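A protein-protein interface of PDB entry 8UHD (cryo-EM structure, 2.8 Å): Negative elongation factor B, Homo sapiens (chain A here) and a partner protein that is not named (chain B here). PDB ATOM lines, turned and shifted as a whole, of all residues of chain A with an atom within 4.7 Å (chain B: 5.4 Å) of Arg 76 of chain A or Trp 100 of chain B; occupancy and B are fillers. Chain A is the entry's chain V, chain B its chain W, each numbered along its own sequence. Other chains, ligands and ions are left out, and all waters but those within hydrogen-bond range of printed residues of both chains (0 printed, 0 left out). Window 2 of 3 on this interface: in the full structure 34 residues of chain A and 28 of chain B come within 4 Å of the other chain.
The backbone carbonyl oxygen (O) of Trp 100 of chain B sits close to the side-chain amide oxygen (OE1) of Gln 103 of chain B, 2.9 Å away. The guanidinium group (NH1) of Arg 76 of chain A is in salt-bridge range of the side-chain carboxylate (OE1) of Glu 83 of chain A (3.7 Å). OG1 of Thr 104 of chain B sits close to O of Trp 100 of chain B (3.4 Å).
CD1 of Leu 97 of chain B touches CB of Leu 69 of chain A (3.4 Å). Leu 69 of chain A touches Ala 98 of chain B. Leu 69 of chain A touches Trp 100 of chain B. Lys 72 of chain A touches Trp 100 of chain B (O to CH2, 3.5 Å). CD2 of Leu 97 of chain B touches CD1 of Leu 73 of chain A, 3.3 Å away. CA of Leu 73 of chain A touches CH2 of Trp 100 of chain B (3.3 Å). Trp 100 of chain B touches Arg 76 of chain A (CZ2 to CB, 3.9 Å).
Of the printed residues of chain B, Leu 69 of chain A touches Leu 97, Ala 98 and Trp 100. Printed residues of chain B within 4 Å of Lys 72 of chain A: Trp 100 (3.5 Å). Of the printed residues of chain B, Leu 73 of chain A touches Leu 97 (3.3 Å) and Trp 100 (3.3 Å). Of the printed residues of chain B, Arg 76 of chain A touches Trp 100 (3.9 Å). Leu 96 of chain B touches none of the printed residues of chain A. Of the printed residues of chain A, Leu 97 of chain B touches Leu 69 (3.4 Å) and Leu 73 (3.3 Å). Trp 100 of chain B touches four residues of chain A. The nearest printed residue of chain A that does not touch Trp 100 of chain B is Leu 74 of chain A (5.6 Å).
Along chain A the printed residues that touch a printed residue of chain B span positions 69 to 76. Printed residues of chain B that touch a printed residue of chain A: Leu 97, Ala 98 and Trp 100. Among the printed residues, 7 pairs touch across the chains. Among the printed residues, no Asp or Glu carboxylate lies within 4 Å of a Lys or Arg side-chain nitrogen of the other chain.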
ATOM      1  N   LEU A  69      -2.863   7.468 -10.972  1.00  0.00           N
ATOM      2  CA  LEU A  69      -2.101   7.491 -12.213  1.00  0.00           C
ATOM      3  C   LEU A  69      -2.133   6.144 -12.941  1.00  0.00           C
ATOM      4  O   LEU A  69      -1.972   6.112 -14.165  1.00  0.00           O
ATOM      5  CB  LEU A  69      -0.669   7.942 -11.921  1.00  0.00           C
ATOM      6  CG  LEU A  69      -0.393   9.448 -11.803  1.00  0.00           C
ATOM      7  CD1 LEU A  69      -1.109  10.101 -10.625  1.00  0.00           C
ATOM      8  CD2 LEU A  69       1.107   9.691 -11.696  1.00  0.00           C
ATOM      9  N   LYS A  72      -5.067   6.479 -14.893  1.00  0.00           N
ATOM     10  CA  LYS A  72      -4.715   7.271 -16.071  1.00  0.00           C
ATOM     11  C   LYS A  72      -4.024   6.413 -17.141  1.00  0.00           C
ATOM     12  O   LYS A  72      -4.237   6.635 -18.337  1.00  0.00           O
ATOM     13  CB  LYS A  72      -3.840   8.463 -15.666  1.00  0.00           C
ATOM     14  CG  LYS A  72      -4.578   9.616 -14.931  1.00  0.00           C
ATOM     15  CD  LYS A  72      -5.720  10.298 -15.713  1.00  0.00           C
ATOM     16  CE  LYS A  72      -5.295  10.863 -17.062  1.00  0.00           C
ATOM     17  NZ  LYS A  72      -4.214  11.879 -16.945  1.00  0.00           N
ATOM     18  N   LEU A  73      -3.180   5.449 -16.735  1.00  0.00           N
ATOM     19  CA  LEU A  73      -2.659   4.435 -17.671  1.00  0.00           C
ATOM     20  C   LEU A  73      -3.778   3.735 -18.421  1.00  0.00           C
ATOM     21  O   LEU A  73      -3.760   3.663 -19.661  1.00  0.00           O
ATOM     22  CB  LEU A  73      -1.787   3.408 -16.933  1.00  0.00           C
ATOM     23  CG  LEU A  73      -0.276   3.594 -16.740  1.00  0.00           C
ATOM     24  CD1 LEU A  73       0.241   2.545 -15.753  1.00  0.00           C
ATOM     25  CD2 LEU A  73       0.473   3.425 -18.064  1.00  0.00           C
ATOM     26  N   LEU A  74      -4.767   3.226 -17.687  1.00  0.00           N
ATOM     27  CA  LEU A  74      -5.856   2.500 -18.335  1.00  0.00           C
ATOM     28  C   LEU A  74      -6.651   3.418 -19.262  1.00  0.00           C
ATOM     29  O   LEU A  74      -7.000   3.031 -20.389  1.00  0.00           O
ATOM     30  CB  LEU A  74      -6.754   1.861 -17.277  1.00  0.00           C
ATOM     31  CG  LEU A  74      -6.061   0.927 -16.268  1.00  0.00           C
ATOM     32  CD1 LEU A  74      -7.111   0.165 -15.495  1.00  0.00           C
ATOM     33  CD2 LEU A  74      -5.029  -0.043 -16.875  1.00  0.00           C
ATOM     34  N   GLU A  75      -6.905   4.654 -18.825  1.00  0.00           N
ATOM     35  CA  GLU A  75      -7.649   5.598 -19.652  1.00  0.00           C
ATOM     36  C   GLU A  75      -6.888   5.948 -20.924  1.00  0.00           C
ATOM     37  O   GLU A  75      -7.486   6.052 -21.999  1.00  0.00           O
ATOM     38  CB  GLU A  75      -7.963   6.872 -18.863  1.00  0.00           C
ATOM     39  CG  GLU A  75      -9.001   6.722 -17.746  1.00  0.00           C
ATOM     40  CD  GLU A  75     -10.372   6.306 -18.243  1.00  0.00           C
ATOM     41  OE1 GLU A  75     -10.734   6.673 -19.380  1.00  0.00           O
ATOM     42  OE2 GLU A  75     -11.086   5.608 -17.493  1.00  0.00           O
ATOM     43  N   ARG A  76      -5.568   6.143 -20.829  1.00  0.00           N
ATOM     44  CA  ARG A  76      -4.821   6.569 -22.007  1.00  0.00           C
ATOM     45  C   ARG A  76      -4.680   5.437 -23.016  1.00  0.00           C
ATOM     46  O   ARG A  76      -4.718   5.683 -24.226  1.00  0.00           O
ATOM     47  CB  ARG A  76      -3.444   7.114 -21.612  1.00  0.00           C
ATOM     48  CG  ARG A  76      -2.643   7.783 -22.760  1.00  0.00           C
ATOM     49  CD  ARG A  76      -3.375   8.974 -23.395  1.00  0.00           C
ATOM     50  NE  ARG A  76      -2.565   9.691 -24.375  1.00  0.00           N
ATOM     51  CZ  ARG A  76      -3.014  10.648 -25.181  1.00  0.00           C
ATOM     52  NH1 ARG A  76      -4.284  11.030 -25.173  1.00  0.00           N
ATOM     53  NH2 ARG A  76      -2.169  11.236 -26.021  1.00  0.00           N
ATOM     54  N   VAL A  77      -4.511   4.192 -22.555  1.00  0.00           N
ATOM     55  CA  VAL A  77      -4.489   3.092 -23.523  1.00  0.00           C
ATOM     56  C   VAL A  77      -5.871   2.919 -24.155  1.00  0.00           C
ATOM     57  O   VAL A  77      -5.990   2.650 -25.362  1.00  0.00           O
ATOM     58  CB  VAL A  77      -3.967   1.784 -22.887  1.00  0.00           C
ATOM     59  CG1 VAL A  77      -4.833   1.305 -21.742  1.00  0.00           C
ATOM     60  CG2 VAL A  77      -3.839   0.685 -23.934  1.00  0.00           C
ATOM     61  N   SER A  78      -6.938   3.106 -23.368  1.00  0.00           N
ATOM     62  CA  SER A  78      -8.284   3.051 -23.935  1.00  0.00           C
ATOM     63  C   SER A  78      -8.486   4.141 -24.983  1.00  0.00           C
ATOM     64  O   SER A  78      -9.137   3.915 -26.010  1.00  0.00           O
ATOM     65  CB  SER A  78      -9.324   3.179 -22.822  1.00  0.00           C
ATOM     66  OG  SER A  78      -9.170   2.150 -21.860  1.00  0.00           O
ATOM     67  N   ALA A  79      -7.937   5.332 -24.737  1.00  0.00           N
ATOM     68  CA  ALA A  79      -8.063   6.424 -25.697  1.00  0.00           C
ATOM     69  C   ALA A  79      -7.242   6.163 -26.954  1.00  0.00           C
ATOM     70  O   ALA A  79      -7.728   6.375 -28.070  1.00  0.00           O
ATOM     71  CB  ALA A  79      -7.636   7.741 -25.048  1.00  0.00           C
ATOM     72  N   ILE A  80      -5.997   5.699 -26.798  1.00  0.00           N
ATOM     73  CA  ILE A  80      -5.150   5.475 -27.963  1.00  0.00           C
ATOM     74  C   ILE A  80      -5.613   4.272 -28.778  1.00  0.00           C
ATOM     75  O   ILE A  80      -5.137   4.100 -29.903  1.00  0.00           O
ATOM     76  CB  ILE A  80      -3.662   5.325 -27.562  1.00  0.00           C
ATOM     77  CG1 ILE A  80      -2.748   5.704 -28.740  1.00  0.00           C
ATOM     78  CG2 ILE A  80      -3.331   3.903 -27.101  1.00  0.00           C
ATOM     79  CD1 ILE A  80      -1.261   5.725 -28.410  1.00  0.00           C
ATOM     80  N   GLU A  83      -7.072   6.050 -31.857  1.00  0.00           N
ATOM     81  CA  GLU A  83      -6.563   7.409 -31.999  1.00  0.00           C
ATOM     82  C   GLU A  83      -5.493   7.439 -33.079  1.00  0.00           C
ATOM     83  O   GLU A  83      -4.509   6.695 -33.001  1.00  0.00           O
ATOM     84  CB  GLU A  83      -5.972   7.914 -30.680  1.00  0.00           C
ATOM     85  CG  GLU A  83      -5.599   9.394 -30.657  1.00  0.00           C
ATOM     86  CD  GLU A  83      -4.802   9.767 -29.423  1.00  0.00           C
ATOM     87  OE1 GLU A  83      -5.074   9.201 -28.344  1.00  0.00           O
ATOM     88  OE2 GLU A  83      -3.900  10.625 -29.533  1.00  0.00           O
ATOM     89  N   ASN B  95       6.553   7.137  -9.502  1.00  0.00           N
ATOM     90  CA  ASN B  95       7.581   7.757 -10.337  1.00  0.00           C
ATOM     91  C   ASN B  95       7.516   7.220 -11.756  1.00  0.00           C
ATOM     92  O   ASN B  95       7.601   7.985 -12.725  1.00  0.00           O
ATOM     93  CB  ASN B  95       8.973   7.520  -9.759  1.00  0.00           C
ATOM     94  CG  ASN B  95       9.072   7.925  -8.324  1.00  0.00           C
ATOM     95  OD1 ASN B  95       8.086   8.353  -7.739  1.00  0.00           O
ATOM     96  ND2 ASN B  95      10.251   7.778  -7.734  1.00  0.00           N
ATOM     97  N   LEU B  96       7.359   5.902 -11.891  1.00  0.00           N
ATOM     98  CA  LEU B  96       7.230   5.303 -13.215  1.00  0.00           C
ATOM     99  C   LEU B  96       5.982   5.812 -13.930  1.00  0.00           C
ATOM    100  O   LEU B  96       6.014   6.084 -15.133  1.00  0.00           O
ATOM    101  CB  LEU B  96       7.221   3.775 -13.108  1.00  0.00           C
ATOM    102  CG  LEU B  96       8.568   3.026 -13.173  1.00  0.00           C
ATOM    103  CD1 LEU B  96       9.251   3.196 -14.530  1.00  0.00           C
ATOM    104  CD2 LEU B  96       9.530   3.422 -12.048  1.00  0.00           C
ATOM    105  N   LEU B  97       4.874   5.972 -13.200  1.00  0.00           N
ATOM    106  CA  LEU B  97       3.662   6.500 -13.830  1.00  0.00           C
ATOM    107  C   LEU B  97       3.839   7.961 -14.255  1.00  0.00           C
ATOM    108  O   LEU B  97       3.406   8.353 -15.341  1.00  0.00           O
ATOM    109  CB  LEU B  97       2.455   6.374 -12.900  1.00  0.00           C
ATOM    110  CG  LEU B  97       2.128   5.048 -12.199  1.00  0.00           C
ATOM    111  CD1 LEU B  97       1.111   5.204 -11.074  1.00  0.00           C
ATOM    112  CD2 LEU B  97       1.638   4.026 -13.180  1.00  0.00           C
ATOM    113  N   ALA B  98       4.455   8.788 -13.417  1.00  0.00           N
ATOM    114  CA  ALA B  98       4.612  10.201 -13.761  1.00  0.00           C
ATOM    115  C   ALA B  98       5.539  10.368 -14.959  1.00  0.00           C
ATOM    116  O   ALA B  98       5.253  11.149 -15.879  1.00  0.00           O
ATOM    117  CB  ALA B  98       5.130  10.982 -12.556  1.00  0.00           C
ATOM    118  N   GLU B  99       6.655   9.635 -14.974  1.00  0.00           N
ATOM    119  CA  GLU B  99       7.541   9.726 -16.129  1.00  0.00           C
ATOM    120  C   GLU B  99       6.912   9.092 -17.363  1.00  0.00           C
ATOM    121  O   GLU B  99       7.224   9.510 -18.482  1.00  0.00           O
ATOM    122  CB  GLU B  99       8.909   9.103 -15.829  1.00  0.00           C
ATOM    123  CG  GLU B  99       8.920   7.613 -15.510  1.00  0.00           C
ATOM    124  CD  GLU B  99       9.010   6.698 -16.731  1.00  0.00           C
ATOM    125  OE1 GLU B  99       9.390   7.165 -17.826  1.00  0.00           O
ATOM    126  OE2 GLU B  99       8.695   5.499 -16.589  1.00  0.00           O
ATOM    127  N   TRP B 100       6.021   8.103 -17.201  1.00  0.00           N
ATOM    128  CA  TRP B 100       5.314   7.610 -18.377  1.00  0.00           C
ATOM    129  C   TRP B 100       4.376   8.676 -18.922  1.00  0.00           C
ATOM    130  O   TRP B 100       4.244   8.823 -20.143  1.00  0.00           O
ATOM    131  CB  TRP B 100       4.547   6.300 -18.102  1.00  0.00           C
ATOM    132  CG  TRP B 100       3.284   6.246 -18.910  1.00  0.00           C
ATOM    133  CD1 TRP B 100       3.171   5.808 -20.188  1.00  0.00           C
ATOM    134  CD2 TRP B 100       1.956   6.561 -18.481  1.00  0.00           C
ATOM    135  NE1 TRP B 100       1.870   5.898 -20.611  1.00  0.00           N
ATOM    136  CE2 TRP B 100       1.103   6.356 -19.575  1.00  0.00           C
ATOM    137  CE3 TRP B 100       1.407   7.022 -17.288  1.00  0.00           C
ATOM    138  CZ2 TRP B 100      -0.254   6.592 -19.503  1.00  0.00           C
ATOM    139  CZ3 TRP B 100       0.058   7.239 -17.227  1.00  0.00           C
ATOM    140  CH2 TRP B 100      -0.741   7.074 -18.326  1.00  0.00           C
ATOM    141  N   LEU B 101       3.697   9.413 -18.035  1.00  0.00           N
ATOM    142  CA  LEU B 101       2.851  10.503 -18.508  1.00  0.00           C
ATOM    143  C   LEU B 101       3.672  11.533 -19.267  1.00  0.00           C
ATOM    144  O   LEU B 101       3.281  11.974 -20.355  1.00  0.00           O
ATOM    145  CB  LEU B 101       2.117  11.204 -17.352  1.00  0.00           C
ATOM    146  CG  LEU B 101       0.741  10.664 -16.966  1.00  0.00           C
ATOM    147  CD1 LEU B 101       0.206  11.121 -15.609  1.00  0.00           C
ATOM    148  CD2 LEU B 101      -0.315  10.863 -18.050  1.00  0.00           C
ATOM    149  N   ILE B 102       4.839  11.887 -18.730  1.00  0.00           N
ATOM    150  CA  ILE B 102       5.704  12.861 -19.390  1.00  0.00           C
ATOM    151  C   ILE B 102       6.165  12.328 -20.743  1.00  0.00           C
ATOM    152  O   ILE B 102       6.266  13.077 -21.722  1.00  0.00           O
ATOM    153  CB  ILE B 102       6.885  13.208 -18.466  1.00  0.00           C
ATOM    154  CG1 ILE B 102       6.377  13.946 -17.215  1.00  0.00           C
ATOM    155  CG2 ILE B 102       7.898  14.076 -19.201  1.00  0.00           C
ATOM    156  CD1 ILE B 102       7.309  13.875 -16.025  1.00  0.00           C
ATOM    157  N   GLN B 103       6.439  11.023 -20.819  1.00  0.00           N
ATOM    158  CA  GLN B 103       6.856  10.396 -22.070  1.00  0.00           C
ATOM    159  C   GLN B 103       5.707  10.270 -23.073  1.00  0.00           C
ATOM    160  O   GLN B 103       5.966  10.131 -24.273  1.00  0.00           O
ATOM    161  CB  GLN B 103       7.493   9.033 -21.746  1.00  0.00           C
ATOM    162  CG  GLN B 103       7.598   8.006 -22.883  1.00  0.00           C
ATOM    163  CD  GLN B 103       6.403   7.066 -22.970  1.00  0.00           C
ATOM    164  OE1 GLN B 103       5.376   7.276 -22.325  1.00  0.00           O
ATOM    165  NE2 GLN B 103       6.543   6.013 -23.765  1.00  0.00           N
ATOM    166  N   THR B 104       4.450  10.341 -22.624  1.00  0.00           N
ATOM    167  CA  THR B 104       3.302  10.300 -23.529  1.00  0.00           C
ATOM    168  C   THR B 104       3.006  11.634 -24.202  1.00  0.00           C
ATOM    169  O   THR B 104       2.050  11.708 -24.982  1.00  0.00           O
ATOM    170  CB  THR B 104       2.033   9.857 -22.791  1.00  0.00           C
ATOM    171  OG1 THR B 104       1.827  10.678 -21.634  1.00  0.00           O
ATOM    172  CG2 THR B 104       2.105   8.430 -22.385  1.00  0.00           C
ATOM    173  N   VAL B 106       2.092  14.248 -22.386  1.00  0.00           N
ATOM    174  CA  VAL B 106       1.386  15.031 -21.382  1.00  0.00           C
ATOM    175  C   VAL B 106       2.390  15.934 -20.683  1.00  0.00           C
ATOM    176  O   VAL B 106       3.443  15.476 -20.221  1.00  0.00           O
ATOM    177  CB  VAL B 106       0.665  14.110 -20.383  1.00  0.00           C
ATOM    178  CG1 VAL B 106       0.161  14.899 -19.171  1.00  0.00           C
ATOM    179  CG2 VAL B 106      -0.481  13.375 -21.068  1.00  0.00           C
